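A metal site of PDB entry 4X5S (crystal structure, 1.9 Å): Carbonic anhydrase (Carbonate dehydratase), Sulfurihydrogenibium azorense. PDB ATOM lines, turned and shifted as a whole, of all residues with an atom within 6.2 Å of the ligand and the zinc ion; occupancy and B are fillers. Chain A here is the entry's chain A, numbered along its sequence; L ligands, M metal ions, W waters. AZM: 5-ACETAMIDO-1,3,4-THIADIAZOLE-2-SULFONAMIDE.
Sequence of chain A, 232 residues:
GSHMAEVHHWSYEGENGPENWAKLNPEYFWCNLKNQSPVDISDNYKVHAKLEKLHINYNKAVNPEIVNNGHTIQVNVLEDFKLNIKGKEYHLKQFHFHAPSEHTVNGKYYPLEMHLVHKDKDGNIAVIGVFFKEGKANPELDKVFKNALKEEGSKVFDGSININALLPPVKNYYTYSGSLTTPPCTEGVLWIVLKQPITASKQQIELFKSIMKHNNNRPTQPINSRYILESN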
ATOM      1  N   SER A  37      -0.234 -24.687 -26.635  1.00  0.00           N
ATOM      2  CA  SER A  37      -0.836 -23.362 -26.549  1.00  0.00           C
ATOM      3  C   SER A  37      -1.452 -23.229 -25.130  1.00  0.00           C
ATOM      4  O   SER A  37      -1.781 -24.224 -24.489  1.00  0.00           O
ATOM      5  CB  SER A  37      -1.924 -23.221 -27.610  1.00  0.00           C
ATOM      6  OG  SER A  37      -1.350 -23.285 -28.912  1.00  0.00           O
ATOM      7  N   GLN A  74     -19.751 -21.530 -23.371  1.00  0.00           N
ATOM      8  CA  GLN A  74     -19.574 -21.820 -24.776  1.00  0.00           C
ATOM      9  C   GLN A  74     -20.878 -21.666 -25.544  1.00  0.00           C
ATOM     10  O   GLN A  74     -21.949 -21.990 -25.016  1.00  0.00           O
ATOM     11  CB  GLN A  74     -19.039 -23.250 -24.907  1.00  0.00           C
ATOM     12  CG  GLN A  74     -18.813 -23.760 -26.310  1.00  0.00           C
ATOM     13  CD  GLN A  74     -18.304 -25.177 -26.295  1.00  0.00           C
ATOM     14  OE1 GLN A  74     -17.461 -25.521 -25.460  1.00  0.00           O
ATOM     15  NE2 GLN A  74     -18.812 -26.019 -27.198  1.00  0.00           N
ATOM     16  N   GLN A  94     -18.176 -23.486 -32.617  1.00  0.00           N
ATOM     17  CA  GLN A  94     -18.553 -22.798 -31.390  1.00  0.00           C
ATOM     18  C   GLN A  94     -17.507 -21.776 -30.999  1.00  0.00           C
ATOM     19  O   GLN A  94     -16.386 -21.791 -31.504  1.00  0.00           O
ATOM     20  CB  GLN A  94     -18.693 -23.799 -30.210  1.00  0.00           C
ATOM     21  CG  GLN A  94     -17.488 -24.765 -30.043  1.00  0.00           C
ATOM     22  CD  GLN A  94     -16.445 -24.347 -28.979  1.00  0.00           C
ATOM     23  OE1 GLN A  94     -16.340 -23.183 -28.592  1.00  0.00           O
ATOM     24  NE2 GLN A  94     -15.647 -25.322 -28.531  1.00  0.00           N
ATOM     25  N   HIS A  96     -16.093 -19.696 -27.285  1.00  0.00           N
ATOM     26  CA  HIS A  96     -16.165 -19.702 -25.836  1.00  0.00           C
ATOM     27  C   HIS A  96     -15.207 -18.666 -25.292  1.00  0.00           C
ATOM     28  O   HIS A  96     -14.513 -18.003 -26.066  1.00  0.00           O
ATOM     29  CB  HIS A  96     -15.806 -21.088 -25.287  1.00  0.00           C
ATOM     30  CG  HIS A  96     -14.447 -21.546 -25.674  1.00  0.00           C
ATOM     31  ND1 HIS A  96     -14.204 -22.278 -26.809  1.00  0.00           N
ATOM     32  CD2 HIS A  96     -13.236 -21.324 -25.102  1.00  0.00           C
ATOM     33  CE1 HIS A  96     -12.901 -22.503 -26.923  1.00  0.00           C
ATOM     34  NE2 HIS A  96     -12.295 -21.934 -25.907  1.00  0.00           N
ATOM     35  N   PHE A  97     -15.142 -18.528 -23.966  1.00  0.00           N
ATOM     36  CA  PHE A  97     -14.317 -17.489 -23.386  1.00  0.00           C
ATOM     37  C   PHE A  97     -13.356 -17.876 -22.266  1.00  0.00           C
ATOM     38  O   PHE A  97     -13.555 -18.871 -21.565  1.00  0.00           O
ATOM     39  CB  PHE A  97     -15.252 -16.391 -22.862  1.00  0.00           C
ATOM     40  CG  PHE A  97     -16.131 -15.798 -23.928  1.00  0.00           C
ATOM     41  CD1 PHE A  97     -15.774 -14.601 -24.550  1.00  0.00           C
ATOM     42  CD2 PHE A  97     -17.297 -16.433 -24.318  1.00  0.00           C
ATOM     43  CE1 PHE A  97     -16.584 -14.049 -25.556  1.00  0.00           C
ATOM     44  CE2 PHE A  97     -18.110 -15.875 -25.316  1.00  0.00           C
ATOM     45  CZ  PHE A  97     -17.743 -14.678 -25.936  1.00  0.00           C
ATOM     46  N   HIS A  98     -12.301 -17.080 -22.127  1.00  0.00           N
ATOM     47  CA  HIS A  98     -11.335 -17.298 -21.059  1.00  0.00           C
ATOM     48  C   HIS A  98     -11.043 -15.950 -20.413  1.00  0.00           C
ATOM     49  O   HIS A  98     -10.875 -14.951 -21.112  1.00  0.00           O
ATOM     50  CB  HIS A  98     -10.020 -17.877 -21.586  1.00  0.00           C
ATOM     51  CG  HIS A  98     -10.147 -19.219 -22.230  1.00  0.00           C
ATOM     52  ND1 HIS A  98      -9.900 -20.401 -21.554  1.00  0.00           N
ATOM     53  CD2 HIS A  98     -10.397 -19.575 -23.519  1.00  0.00           C
ATOM     54  CE1 HIS A  98      -9.984 -21.420 -22.394  1.00  0.00           C
ATOM     55  NE2 HIS A  98     -10.280 -20.944 -23.593  1.00  0.00           N
ATOM     56  N   GLU A 102      -5.715 -16.129 -22.448  1.00  0.00           N
ATOM     57  CA  GLU A 102      -4.782 -17.246 -22.451  1.00  0.00           C
ATOM     58  C   GLU A 102      -3.480 -16.769 -23.107  1.00  0.00           C
ATOM     59  O   GLU A 102      -2.409 -16.922 -22.527  1.00  0.00           O
ATOM     60  CB  GLU A 102      -5.383 -18.427 -23.208  1.00  0.00           C
ATOM     61  CG  GLU A 102      -6.642 -18.930 -22.510  1.00  0.00           C
ATOM     62  CD  GLU A 102      -6.814 -20.414 -22.646  1.00  0.00           C
ATOM     63  OE1 GLU A 102      -7.043 -20.883 -23.791  1.00  0.00           O
ATOM     64  OE2 GLU A 102      -6.707 -21.092 -21.608  1.00  0.00           O
ATOM     65  N   HIS A 115     -12.501 -17.485 -28.135  1.00  0.00           N
ATOM     66  CA  HIS A 115     -11.997 -18.486 -29.065  1.00  0.00           C
ATOM     67  C   HIS A 115     -13.120 -18.987 -29.957  1.00  0.00           C
ATOM     68  O   HIS A 115     -14.155 -19.459 -29.467  1.00  0.00           O
ATOM     69  CB  HIS A 115     -11.362 -19.674 -28.291  1.00  0.00           C
ATOM     70  CG  HIS A 115     -10.063 -19.323 -27.634  1.00  0.00           C
ATOM     71  ND1 HIS A 115      -9.546 -20.048 -26.577  1.00  0.00           N
ATOM     72  CD2 HIS A 115      -9.172 -18.333 -27.871  1.00  0.00           C
ATOM     73  CE1 HIS A 115      -8.404 -19.514 -26.199  1.00  0.00           C
ATOM     74  NE2 HIS A 115      -8.149 -18.472 -26.966  1.00  0.00           N
ATOM     75  N   LEU A 116     -12.916 -18.825 -31.254  1.00  0.00           N
ATOM     76  CA  LEU A 116     -13.827 -19.276 -32.308  1.00  0.00           C
ATOM     77  C   LEU A 116     -13.221 -20.597 -32.793  1.00  0.00           C
ATOM     78  O   LEU A 116     -12.188 -20.606 -33.488  1.00  0.00           O
ATOM     79  CB  LEU A 116     -13.820 -18.258 -33.450  1.00  0.00           C
ATOM     80  CG  LEU A 116     -14.542 -16.939 -33.082  1.00  0.00           C
ATOM     81  CD1 LEU A 116     -13.942 -15.758 -33.851  1.00  0.00           C
ATOM     82  CD2 LEU A 116     -16.042 -17.088 -33.410  1.00  0.00           C
ATOM     83  N   VAL A 117     -13.846 -21.701 -32.443  1.00  0.00           N
ATOM     84  CA  VAL A 117     -13.328 -23.022 -32.778  1.00  0.00           C
ATOM     85  C   VAL A 117     -13.930 -23.590 -34.066  1.00  0.00           C
ATOM     86  O   VAL A 117     -15.133 -23.748 -34.172  1.00  0.00           O
ATOM     87  CB  VAL A 117     -13.602 -23.998 -31.601  1.00  0.00           C
ATOM     88  CG1 VAL A 117     -13.002 -25.358 -31.887  1.00  0.00           C
ATOM     89  CG2 VAL A 117     -12.983 -23.424 -30.299  1.00  0.00           C
ATOM     90  N   ILE A 125      -8.320 -28.744 -36.783  1.00  0.00           N
ATOM     91  CA  ILE A 125      -8.857 -27.618 -36.035  1.00  0.00           C
ATOM     92  C   ILE A 125      -8.130 -26.285 -36.253  1.00  0.00           C
ATOM     93  O   ILE A 125      -6.902 -26.230 -36.356  1.00  0.00           O
ATOM     94  CB  ILE A 125      -8.827 -27.944 -34.525  1.00  0.00           C
ATOM     95  CG1 ILE A 125      -9.659 -29.215 -34.267  1.00  0.00           C
ATOM     96  CG2 ILE A 125      -9.355 -26.768 -33.698  1.00  0.00           C
ATOM     97  CD1 ILE A 125      -9.577 -29.720 -32.857  1.00  0.00           C
ATOM     98  N   VAL A 127      -8.379 -22.264 -34.601  1.00  0.00           N
ATOM     99  CA  VAL A 127      -9.012 -21.437 -33.575  1.00  0.00           C
ATOM    100  C   VAL A 127      -8.616 -19.979 -33.807  1.00  0.00           C
ATOM    101  O   VAL A 127      -7.441 -19.674 -33.996  1.00  0.00           O
ATOM    102  CB  VAL A 127      -8.579 -21.836 -32.143  1.00  0.00           C
ATOM    103  CG1 VAL A 127      -9.328 -20.970 -31.113  1.00  0.00           C
ATOM    104  CG2 VAL A 127      -8.857 -23.326 -31.882  1.00  0.00           C
ATOM    105  N   SER A 179      -1.852 -25.985 -30.069  1.00  0.00           N
ATOM    106  CA  SER A 179      -2.716 -27.034 -29.549  1.00  0.00           C
ATOM    107  C   SER A 179      -3.996 -26.525 -28.940  1.00  0.00           C
ATOM    108  O   SER A 179      -4.252 -25.305 -28.862  1.00  0.00           O
ATOM    109  CB  SER A 179      -1.952 -27.782 -28.446  1.00  0.00           C
ATOM    110  OG  SER A 179      -1.966 -27.029 -27.239  1.00  0.00           O
ATOM    111  N   LEU A 180      -4.823 -27.466 -28.507  1.00  0.00           N
ATOM    112  CA  LEU A 180      -6.042 -27.096 -27.787  1.00  0.00           C
ATOM    113  C   LEU A 180      -5.483 -26.691 -26.423  1.00  0.00           C
ATOM    114  O   LEU A 180      -4.448 -27.212 -26.010  1.00  0.00           O
ATOM    115  CB  LEU A 180      -6.975 -28.305 -27.635  1.00  0.00           C
ATOM    116  CG  LEU A 180      -7.520 -28.870 -28.947  1.00  0.00           C
ATOM    117  CD1 LEU A 180      -8.364 -30.121 -28.642  1.00  0.00           C
ATOM    118  CD2 LEU A 180      -8.364 -27.823 -29.643  1.00  0.00           C
ATOM    119  N   THR A 181      -6.121 -25.750 -25.737  1.00  0.00           N
ATOM    120  CA  THR A 181      -5.609 -25.330 -24.433  1.00  0.00           C
ATOM    121  C   THR A 181      -6.250 -26.032 -23.233  1.00  0.00           C
ATOM    122  O   THR A 181      -6.015 -25.633 -22.102  1.00  0.00           O
ATOM    123  CB  THR A 181      -5.729 -23.824 -24.242  1.00  0.00           C
ATOM    124  OG1 THR A 181      -7.113 -23.463 -24.118  1.00  0.00           O
ATOM    125  CG2 THR A 181      -5.147 -23.110 -25.454  1.00  0.00           C
ATOM    126  N   THR A 182      -7.054 -27.069 -23.474  1.00  0.00           N
ATOM    127  CA  THR A 182      -7.652 -27.867 -22.395  1.00  0.00           C
ATOM    128  C   THR A 182      -7.461 -29.311 -22.846  1.00  0.00           C
ATOM    129  O   THR A 182      -7.386 -29.575 -24.047  1.00  0.00           O
ATOM    130  CB  THR A 182      -9.181 -27.604 -22.207  1.00  0.00           C
ATOM    131  OG1 THR A 182      -9.883 -28.055 -23.354  1.00  0.00           O
ATOM    132  CG2 THR A 182      -9.469 -26.129 -22.039  1.00  0.00           C
ATOM    133  N   PRO A 183      -7.393 -30.258 -21.895  1.00  0.00           N
ATOM    134  CA  PRO A 183      -7.202 -31.673 -22.228  1.00  0.00           C
ATOM    135  C   PRO A 183      -8.163 -32.090 -23.333  1.00  0.00           C
ATOM    136  O   PRO A 183      -9.304 -31.657 -23.329  1.00  0.00           O
ATOM    137  CB  PRO A 183      -7.480 -32.387 -20.909  1.00  0.00           C
ATOM    138  CG  PRO A 183      -7.028 -31.386 -19.883  1.00  0.00           C
ATOM    139  CD  PRO A 183      -7.557 -30.070 -20.441  1.00  0.00           C
ATOM    140  N   PRO A 184      -7.737 -32.961 -24.261  1.00  0.00           N
ATOM    141  CA  PRO A 184      -6.413 -33.601 -24.346  1.00  0.00           C
ATOM    142  C   PRO A 184      -5.234 -32.787 -24.894  1.00  0.00           C
ATOM    143  O   PRO A 184      -4.143 -33.332 -25.095  1.00  0.00           O
ATOM    144  CB  PRO A 184      -6.714 -34.834 -25.186  1.00  0.00           C
ATOM    145  CG  PRO A 184      -7.707 -34.319 -26.154  1.00  0.00           C
ATOM    146  CD  PRO A 184      -8.638 -33.486 -25.299  1.00  0.00           C
ATOM    147  N   VAL A 189      -2.978 -27.853 -34.161  1.00  0.00           N
ATOM    148  CA  VAL A 189      -4.015 -26.827 -34.224  1.00  0.00           C
ATOM    149  C   VAL A 189      -3.491 -25.560 -34.911  1.00  0.00           C
ATOM    150  O   VAL A 189      -2.367 -25.135 -34.649  1.00  0.00           O
ATOM    151  CB  VAL A 189      -4.521 -26.426 -32.798  1.00  0.00           C
ATOM    152  CG1 VAL A 189      -5.534 -25.269 -32.895  1.00  0.00           C
ATOM    153  CG2 VAL A 189      -5.168 -27.659 -32.118  1.00  0.00           C
ATOM    154  N   TRP A 191      -3.575 -21.792 -35.052  1.00  0.00           N
ATOM    155  CA  TRP A 191      -3.987 -20.647 -34.271  1.00  0.00           C
ATOM    156  C   TRP A 191      -3.882 -19.354 -35.102  1.00  0.00           C
ATOM    157  O   TRP A 191      -2.904 -19.132 -35.820  1.00  0.00           O
ATOM    158  CB  TRP A 191      -3.136 -20.494 -33.003  1.00  0.00           C
ATOM    159  CG  TRP A 191      -3.659 -21.300 -31.849  1.00  0.00           C
ATOM    160  CD1 TRP A 191      -3.263 -22.556 -31.479  1.00  0.00           C
ATOM    161  CD2 TRP A 191      -4.728 -20.945 -30.979  1.00  0.00           C
ATOM    162  NE1 TRP A 191      -4.042 -23.018 -30.431  1.00  0.00           N
ATOM    163  CE2 TRP A 191      -4.955 -22.040 -30.105  1.00  0.00           C
ATOM    164  CE3 TRP A 191      -5.538 -19.797 -30.852  1.00  0.00           C
ATOM    165  CZ2 TRP A 191      -5.943 -22.031 -29.125  1.00  0.00           C
ATOM    166  CZ3 TRP A 191      -6.516 -19.779 -29.876  1.00  0.00           C
ATOM    167  CH2 TRP A 191      -6.717 -20.890 -29.022  1.00  0.00           C
HETATM  168  C1  AZM L   1     -10.050 -25.625 -26.884  1.00  0.00           C
HETATM  169  C2  AZM L   1     -11.312 -27.553 -26.863  1.00  0.00           C
HETATM  170  C3  AZM L   1     -13.266 -28.669 -27.871  1.00  0.00           C
HETATM  171  C4  AZM L   1     -14.144 -29.856 -27.694  1.00  0.00           C
HETATM  172  N1  AZM L   1      -9.284 -23.298 -25.774  1.00  0.00           N
HETATM  173  N2  AZM L   1     -10.337 -27.597 -25.987  1.00  0.00           N
HETATM  174  N3  AZM L   1      -9.589 -26.459 -26.004  1.00  0.00           N
HETATM  175  N4  AZM L   1     -12.184 -28.603 -26.990  1.00  0.00           N
HETATM  176  O1  AZM L   1      -7.977 -24.342 -27.549  1.00  0.00           O
HETATM  177  O2  AZM L   1     -10.198 -23.370 -28.069  1.00  0.00           O
HETATM  178  O3  AZM L   1     -13.453 -27.807 -28.697  1.00  0.00           O
HETATM  179  S1  AZM L   1      -9.320 -24.051 -27.155  1.00  0.00           S
HETATM  180  S2  AZM L   1     -11.393 -26.105 -27.801  1.00  0.00           S
HETATM  181 ZN    ZN M   1     -10.397 -21.671 -25.499  1.00  0.00          ZN
HETATM  182  O   HOH W   1     -16.941 -28.453 -28.851  1.00  0.00           O
HETATM  183  O   HOH W   2     -10.718 -30.747 -25.438  1.00  0.00           O
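The side-chain hydroxyl of Thr 182 is in hydrogen-bond range of a nitrogen (N2) of the ligand, at 2.7 Å. The backbone NH (N) of Thr 181 sits at hydrogen-bond distance from an oxygen (O1) of the ligand (3.0 Å). The side-chain hydroxyl of Thr 181 sits close to a nitrogen (N1) of the ligand, 2.7 Å away. NE2 of Gln 94 sits at hydrogen-bond distance from O3 of the ligand.
The side-chain amide oxygen (OE1) of Gln 94 is in hydrogen-bond range of a ring nitrogen (ND1) of His 96 (2.9 Å). A ring nitrogen (ND1) of His 98 sits at hydrogen-bond distance from the side-chain carboxylate (OE2) of Glu 102 (3.3 Å). The side-chain carboxylate of Glu 102 lies within hydrogen-bond range of the side-chain hydroxyl of Thr 181, 2.6 Å away. N of Val 117 sits at hydrogen-bond distance from O of Gln 94 (2.7 Å). The backbone carbonyl oxygen (O) of Ser 179 is in hydrogen-bond range of the indole nitrogen (NE1) of Trp 191 (2.8 Å). The indole nitrogen of Trp 191 sits at hydrogen-bond distance from the side-chain hydroxyl of Ser 37 (3.1 Å).
Glu 102 touches the ligand (OE1 to N1, 3.8 Å). CG2 of Val 117 touches O2 of the ligand, 3.6 Å away. Val 127 touches the ligand. Leu 180 touches the ligand. CZ2 of Trp 191 touches O1 of the ligand, at 3.5 Å. Hydrophobic or aromatic side chains that line the ligand: His 96, His 98, His 115, Val 117, Val 127, Leu 180 and Trp 191. 11 residues have an atom within 4 Å of the ligand: Gln 94, His 96, His 98, Glu 102, His 115, Val 117, Val 127, Leu 180, Thr 181, Thr 182 and Trp 191. Along chain A the residues within 4 Å of the ligand span positions 94 to 191. The nearest printed residue that does not touch the ligand is Ser 179 (4.1 Å).
Residues that only touch the zinc ion: Glu 102 and Thr 181. Five residues have an atom within 4 Å of the zinc ion: His 96, His 98, Glu 102, His 115 and Thr 181. The nearest printed residue that does not touch the zinc ion is Trp 191 (5.2 Å).
The zinc ion is bound by a ring nitrogen (NE2) of His 96, a nitrogen (N1) of the ligand, a ring nitrogen (NE2) of His 98 and a ring nitrogen (ND1) of His 115. The zinc ion has four donor atoms within binding distance.
Water W2 lies within hydrogen-bond range of O of Pro 183 and N4 of the ligand. Water W1 lies within hydrogen-bond range of the side-chain amide nitrogen (NE2) of Gln 94 and the side-chain amide nitrogen (NE2) of Gln 74.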
